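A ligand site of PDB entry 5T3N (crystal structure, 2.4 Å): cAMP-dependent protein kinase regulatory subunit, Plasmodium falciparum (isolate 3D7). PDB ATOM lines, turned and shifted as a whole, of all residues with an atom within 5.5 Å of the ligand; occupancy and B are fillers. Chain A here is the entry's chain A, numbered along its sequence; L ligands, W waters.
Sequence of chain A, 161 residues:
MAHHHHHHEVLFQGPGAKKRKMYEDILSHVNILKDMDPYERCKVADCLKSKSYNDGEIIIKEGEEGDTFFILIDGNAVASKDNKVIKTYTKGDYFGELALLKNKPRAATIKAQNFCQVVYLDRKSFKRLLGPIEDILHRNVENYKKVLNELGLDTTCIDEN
OH of Tyr 144 sits at hydrogen-bond distance from O4 of the ligand (3.5 Å). S1 of the ligand sits close to N of Ala 107 (3.0 Å). An oxygen (O4) of the ligand is in hydrogen-bond range of the side-chain carboxylate (OE1) of Glu 97, at 2.7 Å. An oxygen (O1) of the ligand is in hydrogen-bond range of the guanidinium group of Arg 106, at 3.1 Å. N of Gly 96 sits at hydrogen-bond distance from O4 of the ligand (3.0 Å). O1 of the ligand sits at hydrogen-bond distance from N of Leu 98 (3.4 Å). O1 of the ligand sits at hydrogen-bond distance from N of Ala 99 (2.7 Å).
The backbone carbonyl oxygen (O) of Lys 87 is in hydrogen-bond range of the backbone NH (N) of Ala 79 (2.7 Å). OE2 of Glu 97 lies within hydrogen-bond range of OH of Tyr 144, at 2.5 Å. N of Ile 86 is in hydrogen-bond range of O of Ala 79 (2.8 Å). NH1 of Arg 106 lies within hydrogen-bond range of O of Gly 96 (2.8 Å). N of Ile 110 sits at hydrogen-bond distance from O of Ile 60.
Ile 60 touches the ligand (CG2 to O2, 3.7 Å). Ile 86 touches the ligand. Lys 87 touches the ligand. OH of Tyr 89 touches C10 of the ligand (2.9 Å). CA of Phe 95 touches O4 of the ligand (3.5 Å). Ala 108 touches the ligand (O to C5, 3.6 Å). Ile 110 touches the ligand (CD1 to O3, 3.3 Å). Val 147 touches the ligand (CB to N3, 3.9 Å). Leu 148 touches the ligand (CD1 to N4, 3.5 Å). Ile 158 touches the ligand. Hydrophobic or aromatic side chains that line the ligand: Ile 60, Ile 86, Phe 95, Leu 98, Ala 99, Ala 107, Ala 108, Ile 110, Tyr 144, Val 147, Leu 148 and Ile 158. Along chain A the residues within 4 Å of the ligand span positions 60 to 158.
Water W1 bridges a nitrogen (N3) of the ligand (2.8 Å) and the backbone carbonyl oxygen of Ile 86 (2.8 Å).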
ATOM      1  N   ILE A  60     -18.226  22.475 -11.376  1.00  0.00           N
ATOM      2  CA  ILE A  60     -18.630  21.360 -12.210  1.00  0.00           C
ATOM      3  C   ILE A  60     -19.967  21.712 -12.794  1.00  0.00           C
ATOM      4  O   ILE A  60     -20.860  22.155 -12.056  1.00  0.00           O
ATOM      5  CB  ILE A  60     -18.674  20.056 -11.383  1.00  0.00           C
ATOM      6  CG1 ILE A  60     -17.264  19.572 -11.097  1.00  0.00           C
ATOM      7  CG2 ILE A  60     -19.508  18.963 -12.101  1.00  0.00           C
ATOM      8  CD1 ILE A  60     -17.191  18.373 -10.173  1.00  0.00           C
ATOM      9  N   ALA A  79     -23.619  21.519  -4.130  1.00  0.00           N
ATOM     10  CA  ALA A  79     -24.032  20.731  -5.288  1.00  0.00           C
ATOM     11  C   ALA A  79     -25.539  20.719  -5.439  1.00  0.00           C
ATOM     12  O   ALA A  79     -26.280  20.441  -4.487  1.00  0.00           O
ATOM     13  CB  ALA A  79     -23.510  19.343  -5.172  1.00  0.00           C
ATOM     14  N   ILE A  86     -28.427  19.101  -3.212  1.00  0.00           N
ATOM     15  CA  ILE A  86     -28.238  17.714  -2.851  1.00  0.00           C
ATOM     16  C   ILE A  86     -27.058  17.574  -1.917  1.00  0.00           C
ATOM     17  O   ILE A  86     -26.929  16.541  -1.261  1.00  0.00           O
ATOM     18  CB  ILE A  86     -28.046  16.828  -4.108  1.00  0.00           C
ATOM     19  CG1 ILE A  86     -26.772  17.241  -4.879  1.00  0.00           C
ATOM     20  CG2 ILE A  86     -29.246  16.932  -5.045  1.00  0.00           C
ATOM     21  CD1 ILE A  86     -26.510  16.395  -6.150  1.00  0.00           C
ATOM     22  N   LYS A  87     -26.184  18.581  -1.821  1.00  0.00           N
ATOM     23  CA  LYS A  87     -25.077  18.480  -0.857  1.00  0.00           C
ATOM     24  C   LYS A  87     -24.373  19.841  -0.684  1.00  0.00           C
ATOM     25  O   LYS A  87     -24.130  20.577  -1.660  1.00  0.00           O
ATOM     26  CB  LYS A  87     -24.101  17.363  -1.233  1.00  0.00           C
ATOM     27  CG  LYS A  87     -23.055  17.082  -0.174  1.00  0.00           C
ATOM     28  CD  LYS A  87     -22.860  15.552  -0.089  1.00  0.00           C
ATOM     29  CE  LYS A  87     -22.058  15.073   1.143  1.00  0.00           C
ATOM     30  NZ  LYS A  87     -21.630  16.180   2.058  1.00  0.00           N
ATOM     31  N   TYR A  89     -20.791  21.587   0.705  1.00  0.00           N
ATOM     32  CA  TYR A  89     -19.407  21.170   0.903  1.00  0.00           C
ATOM     33  C   TYR A  89     -18.579  22.180   1.686  1.00  0.00           C
ATOM     34  O   TYR A  89     -18.722  23.409   1.527  1.00  0.00           O
ATOM     35  CB  TYR A  89     -18.717  20.933  -0.458  1.00  0.00           C
ATOM     36  CG  TYR A  89     -19.177  19.701  -1.251  1.00  0.00           C
ATOM     37  CD1 TYR A  89     -18.968  18.429  -0.770  1.00  0.00           C
ATOM     38  CD2 TYR A  89     -19.877  19.834  -2.469  1.00  0.00           C
ATOM     39  CE1 TYR A  89     -19.365  17.315  -1.482  1.00  0.00           C
ATOM     40  CE2 TYR A  89     -20.287  18.721  -3.191  1.00  0.00           C
ATOM     41  CZ  TYR A  89     -20.020  17.456  -2.684  1.00  0.00           C
ATOM     42  OH  TYR A  89     -20.394  16.310  -3.358  1.00  0.00           O
ATOM     43  N   TYR A  94     -14.619  15.921  -0.716  1.00  0.00           N
ATOM     44  CA  TYR A  94     -14.153  15.617  -2.062  1.00  0.00           C
ATOM     45  C   TYR A  94     -15.396  15.502  -2.930  1.00  0.00           C
ATOM     46  O   TYR A  94     -16.500  15.302  -2.424  1.00  0.00           O
ATOM     47  CB  TYR A  94     -13.313  14.332  -2.141  1.00  0.00           C
ATOM     48  CG  TYR A  94     -14.151  13.085  -1.937  1.00  0.00           C
ATOM     49  CD1 TYR A  94     -14.690  12.394  -3.013  1.00  0.00           C
ATOM     50  CD2 TYR A  94     -14.219  12.510  -0.682  1.00  0.00           C
ATOM     51  CE1 TYR A  94     -15.443  11.235  -2.814  1.00  0.00           C
ATOM     52  CE2 TYR A  94     -14.932  11.342  -0.470  1.00  0.00           C
ATOM     53  CZ  TYR A  94     -15.557  10.705  -1.546  1.00  0.00           C
ATOM     54  OH  TYR A  94     -16.305   9.554  -1.363  1.00  0.00           O
ATOM     55  N   PHE A  95     -15.217  15.695  -4.232  1.00  0.00           N
ATOM     56  CA  PHE A  95     -16.320  15.553  -5.150  1.00  0.00           C
ATOM     57  C   PHE A  95     -15.772  15.453  -6.560  1.00  0.00           C
ATOM     58  O   PHE A  95     -14.627  15.833  -6.812  1.00  0.00           O
ATOM     59  CB  PHE A  95     -17.288  16.741  -5.114  1.00  0.00           C
ATOM     60  CG  PHE A  95     -16.627  18.097  -5.162  1.00  0.00           C
ATOM     61  CD1 PHE A  95     -16.520  18.874  -4.013  1.00  0.00           C
ATOM     62  CD2 PHE A  95     -16.171  18.627  -6.382  1.00  0.00           C
ATOM     63  CE1 PHE A  95     -15.945  20.136  -4.063  1.00  0.00           C
ATOM     64  CE2 PHE A  95     -15.628  19.878  -6.447  1.00  0.00           C
ATOM     65  CZ  PHE A  95     -15.503  20.647  -5.285  1.00  0.00           C
ATOM     66  N   GLY A  96     -16.635  15.047  -7.493  1.00  0.00           N
ATOM     67  CA  GLY A  96     -16.254  14.909  -8.885  1.00  0.00           C
ATOM     68  C   GLY A  96     -15.694  13.556  -9.217  1.00  0.00           C
ATOM     69  O   GLY A  96     -15.211  13.337 -10.326  1.00  0.00           O
ATOM     70  N   GLU A  97     -15.803  12.610  -8.287  1.00  0.00           N
ATOM     71  CA  GLU A  97     -15.298  11.261  -8.528  1.00  0.00           C
ATOM     72  C   GLU A  97     -16.184  10.352  -9.393  1.00  0.00           C
ATOM     73  O   GLU A  97     -15.675   9.450 -10.076  1.00  0.00           O
ATOM     74  CB  GLU A  97     -15.038  10.578  -7.182  1.00  0.00           C
ATOM     75  CG  GLU A  97     -16.266   9.873  -6.533  1.00  0.00           C
ATOM     76  CD  GLU A  97     -17.288  10.857  -5.929  1.00  0.00           C
ATOM     77  OE1 GLU A  97     -17.182  12.080  -6.156  1.00  0.00           O
ATOM     78  OE2 GLU A  97     -18.223  10.376  -5.222  1.00  0.00           O
ATOM     79  N   LEU A  98     -17.497  10.590  -9.402  1.00  0.00           N
ATOM     80  CA  LEU A  98     -18.406   9.623 -10.011  1.00  0.00           C
ATOM     81  C   LEU A  98     -18.193   9.524 -11.526  1.00  0.00           C
ATOM     82  O   LEU A  98     -18.131   8.414 -12.075  1.00  0.00           O
ATOM     83  CB  LEU A  98     -19.839  10.017  -9.699  1.00  0.00           C
ATOM     84  CG  LEU A  98     -20.854   8.961 -10.077  1.00  0.00           C
ATOM     85  CD1 LEU A  98     -20.611   7.663  -9.282  1.00  0.00           C
ATOM     86  CD2 LEU A  98     -22.173   9.540  -9.777  1.00  0.00           C
ATOM     87  N   ALA A  99     -18.002  10.665 -12.188  1.00  0.00           N
ATOM     88  CA  ALA A  99     -17.766  10.691 -13.644  1.00  0.00           C
ATOM     89  C   ALA A  99     -16.458   9.938 -13.990  1.00  0.00           C
ATOM     90  O   ALA A  99     -16.322   9.371 -15.081  1.00  0.00           O
ATOM     91  CB  ALA A  99     -17.706  12.110 -14.149  1.00  0.00           C
ATOM     92  N   LEU A 100     -15.474   9.995 -13.100  1.00  0.00           N
ATOM     93  CA  LEU A 100     -14.203   9.304 -13.329  1.00  0.00           C
ATOM     94  C   LEU A 100     -14.390   7.796 -13.154  1.00  0.00           C
ATOM     95  O   LEU A 100     -13.792   6.997 -13.895  1.00  0.00           O
ATOM     96  CB  LEU A 100     -13.097   9.830 -12.427  1.00  0.00           C
ATOM     97  CG  LEU A 100     -13.012  11.344 -12.430  1.00  0.00           C
ATOM     98  CD1 LEU A 100     -11.887  11.811 -11.544  1.00  0.00           C
ATOM     99  CD2 LEU A 100     -12.815  11.836 -13.864  1.00  0.00           C
ATOM    100  N   PRO A 105     -21.103  11.470 -18.139  1.00  0.00           N
ATOM    101  CA  PRO A 105     -21.033  12.914 -17.870  1.00  0.00           C
ATOM    102  C   PRO A 105     -21.313  13.272 -16.405  1.00  0.00           C
ATOM    103  O   PRO A 105     -21.854  12.451 -15.649  1.00  0.00           O
ATOM    104  CB  PRO A 105     -22.110  13.491 -18.786  1.00  0.00           C
ATOM    105  CG  PRO A 105     -23.032  12.370 -19.069  1.00  0.00           C
ATOM    106  CD  PRO A 105     -22.129  11.160 -19.134  1.00  0.00           C
ATOM    107  N   ARG A 106     -20.867  14.460 -15.993  1.00  0.00           N
ATOM    108  CA  ARG A 106     -21.191  15.000 -14.687  1.00  0.00           C
ATOM    109  C   ARG A 106     -22.701  14.923 -14.388  1.00  0.00           C
ATOM    110  O   ARG A 106     -23.540  15.336 -15.212  1.00  0.00           O
ATOM    111  CB  ARG A 106     -20.739  16.469 -14.610  1.00  0.00           C
ATOM    112  CG  ARG A 106     -19.232  16.680 -14.854  1.00  0.00           C
ATOM    113  CD  ARG A 106     -18.359  16.054 -13.776  1.00  0.00           C
ATOM    114  NE  ARG A 106     -17.031  16.659 -13.749  1.00  0.00           N
ATOM    115  CZ  ARG A 106     -16.025  16.229 -12.982  1.00  0.00           C
ATOM    116  NH1 ARG A 106     -16.240  15.210 -12.144  1.00  0.00           N
ATOM    117  NH2 ARG A 106     -14.821  16.830 -13.013  1.00  0.00           N
ATOM    118  N   ALA A 107     -23.029  14.395 -13.221  1.00  0.00           N
ATOM    119  CA  ALA A 107     -24.424  14.129 -12.877  1.00  0.00           C
ATOM    120  C   ALA A 107     -25.031  15.306 -12.127  1.00  0.00           C
ATOM    121  O   ALA A 107     -26.229  15.312 -11.855  1.00  0.00           O
ATOM    122  CB  ALA A 107     -24.542  12.861 -12.075  1.00  0.00           C
ATOM    123  N   ALA A 108     -24.219  16.283 -11.753  1.00  0.00           N
ATOM    124  CA  ALA A 108     -24.716  17.388 -10.938  1.00  0.00           C
ATOM    125  C   ALA A 108     -23.825  18.605 -11.108  1.00  0.00           C
ATOM    126  O   ALA A 108     -22.693  18.510 -11.600  1.00  0.00           O
ATOM    127  CB  ALA A 108     -24.768  16.975  -9.464  1.00  0.00           C
ATOM    128  N   THR A 109     -24.341  19.761 -10.724  1.00  0.00           N
ATOM    129  CA  THR A 109     -23.604  21.009 -10.720  1.00  0.00           C
ATOM    130  C   THR A 109     -23.134  21.442  -9.350  1.00  0.00           C
ATOM    131  O   THR A 109     -23.904  21.428  -8.374  1.00  0.00           O
ATOM    132  CB  THR A 109     -24.436  22.116 -11.349  1.00  0.00           C
ATOM    133  OG1 THR A 109     -24.574  21.840 -12.740  1.00  0.00           O
ATOM    134  CG2 THR A 109     -23.734  23.444 -11.193  1.00  0.00           C
ATOM    135  N   ILE A 110     -21.855  21.822  -9.284  1.00  0.00           N
ATOM    136  CA  ILE A 110     -21.246  22.337  -8.065  1.00  0.00           C
ATOM    137  C   ILE A 110     -20.692  23.765  -8.255  1.00  0.00           C
ATOM    138  O   ILE A 110     -19.911  24.033  -9.193  1.00  0.00           O
ATOM    139  CB  ILE A 110     -20.162  21.391  -7.590  1.00  0.00           C
ATOM    140  CG1 ILE A 110     -20.812  20.028  -7.292  1.00  0.00           C
ATOM    141  CG2 ILE A 110     -19.443  21.934  -6.325  1.00  0.00           C
ATOM    142  CD1 ILE A 110     -19.820  18.903  -6.968  1.00  0.00           C
ATOM    143  N   ASN A 143     -25.154   6.163  -0.840  1.00  0.00           N
ATOM    144  CA  ASN A 143     -25.740   7.259  -0.128  1.00  0.00           C
ATOM    145  C   ASN A 143     -26.220   8.348  -1.084  1.00  0.00           C
ATOM    146  O   ASN A 143     -27.169   9.105  -0.751  1.00  0.00           O
ATOM    147  CB  ASN A 143     -24.726   7.863   0.829  1.00  0.00           C
ATOM    148  CG  ASN A 143     -24.435   6.951   1.998  1.00  0.00           C
ATOM    149  OD1 ASN A 143     -25.174   5.996   2.250  1.00  0.00           O
ATOM    150  ND2 ASN A 143     -23.336   7.217   2.696  1.00  0.00           N
ATOM    151  N   TYR A 144     -25.581   8.452  -2.267  1.00  0.00           N
ATOM    152  CA  TYR A 144     -26.082   9.411  -3.244  1.00  0.00           C
ATOM    153  C   TYR A 144     -27.506   9.047  -3.682  1.00  0.00           C
ATOM    154  O   TYR A 144     -28.298   9.926  -4.016  1.00  0.00           O
ATOM    155  CB  TYR A 144     -25.194   9.452  -4.489  1.00  0.00           C
ATOM    156  CG  TYR A 144     -23.818  10.039  -4.298  1.00  0.00           C
ATOM    157  CD1 TYR A 144     -23.587  11.073  -3.401  1.00  0.00           C
ATOM    158  CD2 TYR A 144     -22.747   9.576  -5.059  1.00  0.00           C
ATOM    159  CE1 TYR A 144     -22.305  11.598  -3.240  1.00  0.00           C
ATOM    160  CE2 TYR A 144     -21.472  10.080  -4.909  1.00  0.00           C
ATOM    161  CZ  TYR A 144     -21.259  11.103  -4.017  1.00  0.00           C
ATOM    162  OH  TYR A 144     -19.970  11.607  -3.857  1.00  0.00           O
ATOM    163  N   VAL A 147     -30.297  10.369  -1.445  1.00  0.00           N
ATOM    164  CA  VAL A 147     -30.647  11.747  -1.634  1.00  0.00           C
ATOM    165  C   VAL A 147     -31.412  11.985  -2.948  1.00  0.00           C
ATOM    166  O   VAL A 147     -32.423  12.702  -2.961  1.00  0.00           O
ATOM    167  CB  VAL A 147     -29.342  12.619  -1.686  1.00  0.00           C
ATOM    168  CG1 VAL A 147     -29.651  14.045  -2.071  1.00  0.00           C
ATOM    169  CG2 VAL A 147     -28.549  12.563  -0.378  1.00  0.00           C
ATOM    170  N   LEU A 148     -31.018  11.303  -4.017  1.00  0.00           N
ATOM    171  CA  LEU A 148     -31.685  11.443  -5.308  1.00  0.00           C
ATOM    172  C   LEU A 148     -33.139  11.000  -5.118  1.00  0.00           C
ATOM    173  O   LEU A 148     -34.083  11.644  -5.582  1.00  0.00           O
ATOM    174  CB  LEU A 148     -30.933  10.693  -6.410  1.00  0.00           C
ATOM    175  CG  LEU A 148     -29.557  11.387  -6.577  1.00  0.00           C
ATOM    176  CD1 LEU A 148     -28.591  10.690  -7.538  1.00  0.00           C
ATOM    177  CD2 LEU A 148     -29.712  12.843  -7.009  1.00  0.00           C
ATOM    178  N   CYS A 157     -28.322   8.246 -13.807  1.00  0.00           N
ATOM    179  CA  CYS A 157     -26.923   8.677 -13.887  1.00  0.00           C
ATOM    180  C   CYS A 157     -25.974   7.850 -13.026  1.00  0.00           C
ATOM    181  O   CYS A 157     -24.761   7.847 -13.232  1.00  0.00           O
ATOM    182  CB  CYS A 157     -26.909  10.151 -13.494  1.00  0.00           C
ATOM    183  SG  CYS A 157     -27.523  10.438 -11.804  1.00  0.00           S
ATOM    184  N   ILE A 158     -26.521   7.182 -12.022  1.00  0.00           N
ATOM    185  CA  ILE A 158     -25.788   6.257 -11.165  1.00  0.00           C
ATOM    186  C   ILE A 158     -25.842   4.793 -11.571  1.00  0.00           C
ATOM    187  O   ILE A 158     -24.823   4.124 -11.718  1.00  0.00           O
ATOM    188  CB  ILE A 158     -26.269   6.358  -9.748  1.00  0.00           C
ATOM    189  CG1 ILE A 158     -25.963   7.766  -9.215  1.00  0.00           C
ATOM    190  CG2 ILE A 158     -25.479   5.411  -8.918  1.00  0.00           C
ATOM    191  CD1 ILE A 158     -26.233   7.927  -7.740  1.00  0.00           C
HETATM  192  C1  LIG L   1     -24.740  12.322  -7.423  1.00  0.00           C
HETATM  193  C2  LIG L   1     -23.383  13.817  -6.211  1.00  0.00           C
HETATM  194  C3  LIG L   1     -24.397  13.842  -5.230  1.00  0.00           C
HETATM  195  C4  LIG L   1     -25.584  13.069  -5.348  1.00  0.00           C
HETATM  196  S1  LIG L   1     -21.307  12.884 -11.246  1.00  0.00           S
HETATM  197  P1  LIG L   1     -19.591  13.799 -10.524  1.00  0.00           P
HETATM  198  O1  LIG L   1     -18.508  13.216 -11.371  1.00  0.00           O
HETATM  199  O2  LIG L   1     -19.758  15.525 -10.812  1.00  0.00           O
HETATM  200  C5  LIG L   1     -20.909  16.019  -9.803  1.00  0.00           C
HETATM  201  C6  LIG L   1     -20.485  15.545  -8.495  1.00  0.00           C
HETATM  202  O3  LIG L   1     -21.422  16.062  -7.432  1.00  0.00           O
HETATM  203  C7  LIG L   1     -21.281  14.947  -6.330  1.00  0.00           C
HETATM  204  C8  LIG L   1     -20.516  13.848  -6.905  1.00  0.00           C
HETATM  205  O4  LIG L   1     -19.187  13.889  -6.331  1.00  0.00           O
HETATM  206  C9  LIG L   1     -20.495  14.100  -8.352  1.00  0.00           C
HETATM  207  O5  LIG L   1     -19.428  13.520  -8.997  1.00  0.00           O
HETATM  208  N1  LIG L   1     -22.484  14.621  -5.754  1.00  0.00           N
HETATM  209  C10 LIG L   1     -22.696  15.168  -4.649  1.00  0.00           C
HETATM  210  N2  LIG L   1     -23.901  14.729  -4.206  1.00  0.00           N
HETATM  211  N3  LIG L   1     -26.573  13.115  -4.322  1.00  0.00           N
HETATM  212  N4  LIG L   1     -25.725  12.316  -6.461  1.00  0.00           N
HETATM  213 CL1  LIG L   1     -24.958  11.327  -8.859  1.00  0.00          CL
HETATM  214  N5  LIG L   1     -23.586  13.054  -7.282  1.00  0.00           N
HETATM  215  O   HOH W   1     -25.817  14.034  -1.834  1.00  0.00           O
